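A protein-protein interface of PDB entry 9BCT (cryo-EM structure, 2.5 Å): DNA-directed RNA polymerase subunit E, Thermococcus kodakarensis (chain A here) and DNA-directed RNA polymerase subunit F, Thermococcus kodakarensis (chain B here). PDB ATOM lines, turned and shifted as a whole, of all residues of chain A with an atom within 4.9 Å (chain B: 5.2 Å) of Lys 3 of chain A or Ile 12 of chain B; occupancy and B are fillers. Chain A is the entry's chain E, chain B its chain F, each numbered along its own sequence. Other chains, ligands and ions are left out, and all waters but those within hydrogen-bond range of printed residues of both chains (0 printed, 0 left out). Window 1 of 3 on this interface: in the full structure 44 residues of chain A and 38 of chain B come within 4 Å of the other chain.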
ATOM      1  N   MET A   1      12.846  -7.881  20.767  1.00  0.00           N
ATOM      2  CA  MET A   1      11.718  -8.798  20.884  1.00  0.00           C
ATOM      3  C   MET A   1      10.542  -8.328  20.034  1.00  0.00           C
ATOM      4  O   MET A   1      10.081  -7.195  20.168  1.00  0.00           O
ATOM      5  CB  MET A   1      11.289  -8.937  22.347  1.00  0.00           C
ATOM      6  CG  MET A   1       9.944  -9.622  22.542  1.00  0.00           C
ATOM      7  SD  MET A   1      10.094 -11.385  22.897  1.00  0.00           S
ATOM      8  CE  MET A   1      10.041 -12.079  21.246  1.00  0.00           C
ATOM      9  N   TYR A   2      10.066  -9.207  19.156  1.00  0.00           N
ATOM     10  CA  TYR A   2       8.944  -8.876  18.292  1.00  0.00           C
ATOM     11  C   TYR A   2       7.657  -8.755  19.103  1.00  0.00           C
ATOM     12  O   TYR A   2       7.442  -9.472  20.085  1.00  0.00           O
ATOM     13  CB  TYR A   2       8.783  -9.933  17.201  1.00  0.00           C
ATOM     14  CG  TYR A   2       9.815  -9.838  16.102  1.00  0.00           C
ATOM     15  CD1 TYR A   2       9.590  -9.055  14.978  1.00  0.00           C
ATOM     16  CD2 TYR A   2      11.014 -10.531  16.188  1.00  0.00           C
ATOM     17  CE1 TYR A   2      10.530  -8.966  13.970  1.00  0.00           C
ATOM     18  CE2 TYR A   2      11.962 -10.447  15.186  1.00  0.00           C
ATOM     19  CZ  TYR A   2      11.715  -9.664  14.079  1.00  0.00           C
ATOM     20  OH  TYR A   2      12.653  -9.577  13.077  1.00  0.00           O
ATOM     21  N   LYS A   3       6.795  -7.834  18.678  1.00  0.00           N
ATOM     22  CA  LYS A   3       5.566  -7.522  19.391  1.00  0.00           C
ATOM     23  C   LYS A   3       4.459  -7.220  18.393  1.00  0.00           C
ATOM     24  O   LYS A   3       4.702  -6.613  17.346  1.00  0.00           O
ATOM     25  CB  LYS A   3       5.757  -6.321  20.327  1.00  0.00           C
ATOM     26  CG  LYS A   3       5.622  -6.633  21.803  1.00  0.00           C
ATOM     27  CD  LYS A   3       5.539  -5.348  22.613  1.00  0.00           C
ATOM     28  CE  LYS A   3       5.703  -5.612  24.098  1.00  0.00           C
ATOM     29  NZ  LYS A   3       6.103  -4.384  24.838  1.00  0.00           N
ATOM     30  N   LEU A   4       3.245  -7.652  18.725  1.00  0.00           N
ATOM     31  CA  LEU A   4       2.049  -7.344  17.950  1.00  0.00           C
ATOM     32  C   LEU A   4       1.126  -6.505  18.821  1.00  0.00           C
ATOM     33  O   LEU A   4       0.774  -6.917  19.932  1.00  0.00           O
ATOM     34  CB  LEU A   4       1.348  -8.623  17.489  1.00  0.00           C
ATOM     35  CG  LEU A   4       0.036  -8.458  16.718  1.00  0.00           C
ATOM     36  CD1 LEU A   4       0.208  -7.490  15.561  1.00  0.00           C
ATOM     37  CD2 LEU A   4      -0.467  -9.805  16.224  1.00  0.00           C
ATOM     38  N   LEU A   5       0.738  -5.333  18.323  1.00  0.00           N
ATOM     39  CA  LEU A   5      -0.066  -4.396  19.092  1.00  0.00           C
ATOM     40  C   LEU A   5      -1.323  -4.022  18.323  1.00  0.00           C
ATOM     41  O   LEU A   5      -1.322  -3.948  17.092  1.00  0.00           O
ATOM     42  CB  LEU A   5       0.723  -3.122  19.432  1.00  0.00           C
ATOM     43  CG  LEU A   5       2.209  -3.279  19.754  1.00  0.00           C
ATOM     44  CD1 LEU A   5       2.932  -1.953  19.578  1.00  0.00           C
ATOM     45  CD2 LEU A   5       2.399  -3.812  21.164  1.00  0.00           C
ATOM     46  N   VAL A  74      -0.230  -3.409  14.468  1.00  0.00           N
ATOM     47  CA  VAL A  74       1.142  -2.986  14.210  1.00  0.00           C
ATOM     48  C   VAL A  74       2.083  -4.089  14.669  1.00  0.00           C
ATOM     49  O   VAL A  74       1.963  -4.587  15.795  1.00  0.00           O
ATOM     50  CB  VAL A  74       1.480  -1.665  14.924  1.00  0.00           C
ATOM     51  CG1 VAL A  74       2.708  -1.025  14.297  1.00  0.00           C
ATOM     52  CG2 VAL A  74       0.301  -0.713  14.892  1.00  0.00           C
ATOM     53  N   LEU A  75       3.018  -4.467  13.802  1.00  0.00           N
ATOM     54  CA  LEU A  75       4.099  -5.373  14.160  1.00  0.00           C
ATOM     55  C   LEU A  75       5.352  -4.540  14.393  1.00  0.00           C
ATOM     56  O   LEU A  75       5.840  -3.875  13.471  1.00  0.00           O
ATOM     57  CB  LEU A  75       4.335  -6.412  13.063  1.00  0.00           C
ATOM     58  CG  LEU A  75       5.655  -7.182  13.140  1.00  0.00           C
ATOM     59  CD1 LEU A  75       5.600  -8.238  14.233  1.00  0.00           C
ATOM     60  CD2 LEU A  75       5.991  -7.810  11.797  1.00  0.00           C
ATOM     61  N   VAL A  76       5.859  -4.565  15.626  1.00  0.00           N
ATOM     62  CA  VAL A  76       7.015  -3.773  16.017  1.00  0.00           C
ATOM     63  C   VAL A  76       8.068  -4.700  16.607  1.00  0.00           C
ATOM     64  O   VAL A  76       7.832  -5.886  16.835  1.00  0.00           O
ATOM     65  CB  VAL A  76       6.657  -2.660  17.026  1.00  0.00           C
ATOM     66  CG1 VAL A  76       5.566  -1.761  16.472  1.00  0.00           C
ATOM     67  CG2 VAL A  76       6.235  -3.262  18.354  1.00  0.00           C
ATOM     68  N   TRP A  77       9.248  -4.137  16.852  1.00  0.00           N
ATOM     69  CA  TRP A  77      10.345  -4.857  17.487  1.00  0.00           C
ATOM     70  C   TRP A  77      10.894  -3.996  18.613  1.00  0.00           C
ATOM     71  O   TRP A  77      11.281  -2.846  18.385  1.00  0.00           O
ATOM     72  CB  TRP A  77      11.442  -5.194  16.475  1.00  0.00           C
ATOM     73  CG  TRP A  77      12.497  -6.096  17.021  1.00  0.00           C
ATOM     74  CD1 TRP A  77      12.430  -7.451  17.153  1.00  0.00           C
ATOM     75  CD2 TRP A  77      13.782  -5.707  17.517  1.00  0.00           C
ATOM     76  NE1 TRP A  77      13.594  -7.931  17.698  1.00  0.00           N
ATOM     77  CE2 TRP A  77      14.441  -6.881  17.931  1.00  0.00           C
ATOM     78  CE3 TRP A  77      14.440  -4.481  17.650  1.00  0.00           C
ATOM     79  CZ2 TRP A  77      15.724  -6.864  18.468  1.00  0.00           C
ATOM     80  CZ3 TRP A  77      15.714  -4.468  18.183  1.00  0.00           C
ATOM     81  CH2 TRP A  77      16.342  -5.650  18.586  1.00  0.00           C
ATOM     82  N   GLU A  78      10.930  -4.550  19.818  1.00  0.00           N
ATOM     83  CA  GLU A  78      11.371  -3.814  21.001  1.00  0.00           C
ATOM     84  C   GLU A  78      12.539  -4.530  21.662  1.00  0.00           C
ATOM     85  O   GLU A  78      12.350  -5.622  22.230  1.00  0.00           O
ATOM     86  CB  GLU A  78      10.219  -3.653  21.994  1.00  0.00           C
ATOM     87  CG  GLU A  78      10.550  -2.779  23.192  1.00  0.00           C
ATOM     88  CD  GLU A  78       9.597  -2.994  24.350  1.00  0.00           C
ATOM     89  OE1 GLU A  78       9.163  -4.147  24.559  1.00  0.00           O
ATOM     90  OE2 GLU A  78       9.281  -2.011  25.053  1.00  0.00           O
ATOM     91  N   LYS B   6      -3.117   2.210  23.455  1.00  0.00           N
ATOM     92  CA  LYS B   6      -2.864   0.826  23.082  1.00  0.00           C
ATOM     93  C   LYS B   6      -3.961  -0.059  23.656  1.00  0.00           C
ATOM     94  O   LYS B   6      -4.236  -0.011  24.860  1.00  0.00           O
ATOM     95  CB  LYS B   6      -1.494   0.365  23.585  1.00  0.00           C
ATOM     96  CG  LYS B   6      -0.952  -0.865  22.878  1.00  0.00           C
ATOM     97  CD  LYS B   6       0.556  -0.972  23.033  1.00  0.00           C
ATOM     98  CE  LYS B   6       0.963  -0.971  24.498  1.00  0.00           C
ATOM     99  NZ  LYS B   6       2.284  -1.624  24.708  1.00  0.00           N
ATOM    100  N   GLU B   9      -1.661  -5.794  23.632  1.00  0.00           N
ATOM    101  CA  GLU B   9      -0.228  -5.959  23.432  1.00  0.00           C
ATOM    102  C   GLU B   9       0.120  -7.432  23.575  1.00  0.00           C
ATOM    103  O   GLU B   9      -0.193  -8.050  24.598  1.00  0.00           O
ATOM    104  CB  GLU B   9       0.571  -5.119  24.435  1.00  0.00           C
ATOM    105  CG  GLU B   9       2.023  -5.540  24.581  1.00  0.00           C
ATOM    106  CD  GLU B   9       2.666  -4.980  25.834  1.00  0.00           C
ATOM    107  OE1 GLU B   9       2.584  -5.638  26.892  1.00  0.00           O
ATOM    108  OE2 GLU B   9       3.254  -3.879  25.762  1.00  0.00           O
ATOM    109  N   HIS B  10       0.766  -7.990  22.554  1.00  0.00           N
ATOM    110  CA  HIS B  10       1.128  -9.399  22.535  1.00  0.00           C
ATOM    111  C   HIS B  10       2.588  -9.552  22.139  1.00  0.00           C
ATOM    112  O   HIS B  10       3.074  -8.861  21.239  1.00  0.00           O
ATOM    113  CB  HIS B  10       0.242 -10.190  21.565  1.00  0.00           C
ATOM    114  CG  HIS B  10      -1.222 -10.076  21.854  1.00  0.00           C
ATOM    115  ND1 HIS B  10      -1.822 -10.712  22.920  1.00  0.00           N
ATOM    116  CD2 HIS B  10      -2.208  -9.399  21.217  1.00  0.00           C
ATOM    117  CE1 HIS B  10      -3.113 -10.432  22.927  1.00  0.00           C
ATOM    118  NE2 HIS B  10      -3.373  -9.638  21.905  1.00  0.00           N
ATOM    119  N   TYR B  11       3.282 -10.466  22.814  1.00  0.00           N
ATOM    120  CA  TYR B  11       4.667 -10.796  22.486  1.00  0.00           C
ATOM    121  C   TYR B  11       4.640 -11.875  21.410  1.00  0.00           C
ATOM    122  O   TYR B  11       4.486 -13.061  21.706  1.00  0.00           O
ATOM    123  CB  TYR B  11       5.423 -11.258  23.725  1.00  0.00           C
ATOM    124  CG  TYR B  11       5.759 -10.147  24.692  1.00  0.00           C
ATOM    125  CD1 TYR B  11       4.857  -9.756  25.672  1.00  0.00           C
ATOM    126  CD2 TYR B  11       6.980  -9.489  24.627  1.00  0.00           C
ATOM    127  CE1 TYR B  11       5.159  -8.742  26.560  1.00  0.00           C
ATOM    128  CE2 TYR B  11       7.294  -8.474  25.511  1.00  0.00           C
ATOM    129  CZ  TYR B  11       6.379  -8.104  26.475  1.00  0.00           C
ATOM    130  OH  TYR B  11       6.686  -7.093  27.357  1.00  0.00           O
ATOM    131  N   ILE B  12       4.785 -11.462  20.161  1.00  0.00           N
ATOM    132  CA  ILE B  12       4.660 -12.368  19.027  1.00  0.00           C
ATOM    133  C   ILE B  12       6.009 -13.036  18.785  1.00  0.00           C
ATOM    134  O   ILE B  12       7.061 -12.519  19.174  1.00  0.00           O
ATOM    135  CB  ILE B  12       4.149 -11.607  17.783  1.00  0.00           C
ATOM    136  CG1 ILE B  12       3.565 -12.573  16.752  1.00  0.00           C
ATOM    137  CG2 ILE B  12       5.252 -10.767  17.166  1.00  0.00           C
ATOM    138  CD1 ILE B  12       2.684 -13.643  17.363  1.00  0.00           C
ATOM    139  N   THR B  13       5.982 -14.209  18.152  1.00  0.00           N
ATOM    140  CA  THR B  13       7.181 -15.006  17.952  1.00  0.00           C
ATOM    141  C   THR B  13       7.847 -14.666  16.618  1.00  0.00           C
ATOM    142  O   THR B  13       7.390 -13.806  15.862  1.00  0.00           O
ATOM    143  CB  THR B  13       6.849 -16.497  18.023  1.00  0.00           C
ATOM    144  OG1 THR B  13       6.396 -16.949  16.741  1.00  0.00           O
ATOM    145  CG2 THR B  13       5.764 -16.752  19.059  1.00  0.00           C
ATOM    146  N   ILE B  14       8.954 -15.355  16.332  1.00  0.00           N
ATOM    147  CA  ILE B  14       9.703 -15.105  15.103  1.00  0.00           C
ATOM    148  C   ILE B  14       8.933 -15.602  13.886  1.00  0.00           C
ATOM    149  O   ILE B  14       8.900 -14.936  12.846  1.00  0.00           O
ATOM    150  CB  ILE B  14      11.102 -15.744  15.194  1.00  0.00           C
ATOM    151  CG1 ILE B  14      11.973 -14.984  16.200  1.00  0.00           C
ATOM    152  CG2 ILE B  14      11.765 -15.824  13.818  1.00  0.00           C
ATOM    153  CD1 ILE B  14      12.878 -13.932  15.587  1.00  0.00           C
ATOM    154  N   GLU B  16       5.613 -16.097  13.344  1.00  0.00           N
ATOM    155  CA  GLU B  16       4.452 -15.287  12.992  1.00  0.00           C
ATOM    156  C   GLU B  16       4.874 -13.925  12.453  1.00  0.00           C
ATOM    157  O   GLU B  16       4.238 -13.389  11.537  1.00  0.00           O
ATOM    158  CB  GLU B  16       3.539 -15.130  14.204  1.00  0.00           C
ATOM    159  CG  GLU B  16       2.791 -16.395  14.584  1.00  0.00           C
ATOM    160  CD  GLU B  16       3.316 -17.016  15.864  1.00  0.00           C
ATOM    161  OE1 GLU B  16       4.396 -17.642  15.821  1.00  0.00           O
ATOM    162  OE2 GLU B  16       2.653 -16.878  16.912  1.00  0.00           O
ATOM    163  N   ALA B  17       5.944 -13.352  13.010  1.00  0.00           N
ATOM    164  CA  ALA B  17       6.483 -12.108  12.469  1.00  0.00           C
ATOM    165  C   ALA B  17       6.994 -12.305  11.048  1.00  0.00           C
ATOM    166  O   ALA B  17       6.843 -11.422  10.198  1.00  0.00           O
ATOM    167  CB  ALA B  17       7.595 -11.580  13.373  1.00  0.00           C
ATOM    168  N   LYS B  63       3.591 -22.057  21.664  1.00  0.00           N
ATOM    169  CA  LYS B  63       3.394 -20.927  22.567  1.00  0.00           C
ATOM    170  C   LYS B  63       2.153 -21.117  23.430  1.00  0.00           C
ATOM    171  O   LYS B  63       2.185 -20.849  24.637  1.00  0.00           O
ATOM    172  CB  LYS B  63       3.307 -19.629  21.763  1.00  0.00           C
ATOM    173  CG  LYS B  63       2.581 -18.495  22.467  1.00  0.00           C
ATOM    174  CD  LYS B  63       2.315 -17.338  21.517  1.00  0.00           C
ATOM    175  CE  LYS B  63       3.181 -16.135  21.853  1.00  0.00           C
ATOM    176  NZ  LYS B  63       4.464 -16.529  22.497  1.00  0.00           N
ATOM    177  N   ALA B  79       7.512 -16.767  24.090  1.00  0.00           N
ATOM    178  CA  ALA B  79       8.090 -16.356  22.816  1.00  0.00           C
ATOM    179  C   ALA B  79       9.600 -16.552  22.806  1.00  0.00           C
ATOM    180  O   ALA B  79      10.162 -17.041  21.820  1.00  0.00           O
ATOM    181  CB  ALA B  79       7.735 -14.898  22.525  1.00  0.00           C
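The backbone carbonyl oxygen (O) of Leu 5 of chain A lies within hydrogen-bond range of the backbone NH (N) of Val 74 of chain A, 2.9 Å away. The side-chain carboxylate of Glu 9 of chain B lies within salt-bridge range of the side-chain amino group of Lys 6 of chain B (2.7 Å). The backbone carbonyl oxygen (O) of Val 76 of chain A sits at hydrogen-bond distance from the backbone NH (N) of Lys 3 of chain A (2.9 Å). OE1 of Glu 78 of chain A is in salt-bridge range of NZ of Lys 3 of chain A (3.1 Å). The backbone NH (N) of Met 1 of chain A sits at hydrogen-bond distance from the backbone carbonyl oxygen (O) of Glu 78 of chain A.
N of Ile 12 of chain B is in hydrogen-bond range of O of Tyr 2 of chain A, at 3.3 Å. The backbone NH (N) of Leu 4 of chain A lies within hydrogen-bond range of the backbone carbonyl oxygen (O) of His 10 of chain B, 2.8 Å away. The side-chain amino group of Lys 3 of chain A lies within salt-bridge range of the side-chain carboxylate of Glu 9 of chain B, 3.0 Å away.
CG of Met 1 of chain A touches CD2 of Tyr 11 of chain B, at 3.6 Å. CB of Ala 79 of chain B touches CE of Met 1 of chain A, 3.9 Å away. Tyr 2 of chain A touches Tyr 11 of chain B. Tyr 2 of chain A touches Ile 14 of chain B. CB of Ala 17 of chain B touches CD1 of Tyr 2 of chain A, 3.6 Å away. Lys 3 of chain A touches His 10 of chain B. CE of Lys 3 of chain A touches CZ of Tyr 11 of chain B (3.5 Å). Leu 5 of chain A touches Lys 6 of chain B. Ile 12 of chain B touches Leu 75 of chain A (CG2 to CD1, 3.9 Å). Ala 17 of chain B touches Leu 75 of chain A.
Of the 10 printed residues of chain A, 6 touch a printed residue of chain B. Printed residues of chain A that touch a printed residue of chain B: Met 1, Tyr 2, Lys 3, Leu 4, Leu 5 and Leu 75. Hydrophobic or aromatic side chains of chain A that line the printed part of chain B: Met 1, Tyr 2, Leu 5 and Leu 75. Hydrophobic or aromatic side chains of chain B that line the printed part of chain A: His 10, Tyr 11, Ile 12, Ile 14, Ala 17 and Ala 79. Among the printed residues, 17 pairs touch across the chains.
Lys 3 of chain A touches just these residues of chain B: Glu 9, His 10, Tyr 11 and Ile 12. Ile 12 of chain B touches four residues of chain A. Of the printed residues of chain B, Leu 75 of chain A touches Ile 12 and Ala 17. Of the printed residues of chain A, Ala 79 of chain B touches Met 1. Of the printed residues of chain B, Leu 4 of chain A touches Glu 9 and His 10. Val 76 of chain A touches none of the printed residues of chain B. The nearest residue of chain A that does not touch Ile 12 of chain B is Leu 4 of chain A (4.02 Å). The nearest printed residue of chain A that does not touch Lys 6 of chain B is Lys 3 of chain A (4.7 Å).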
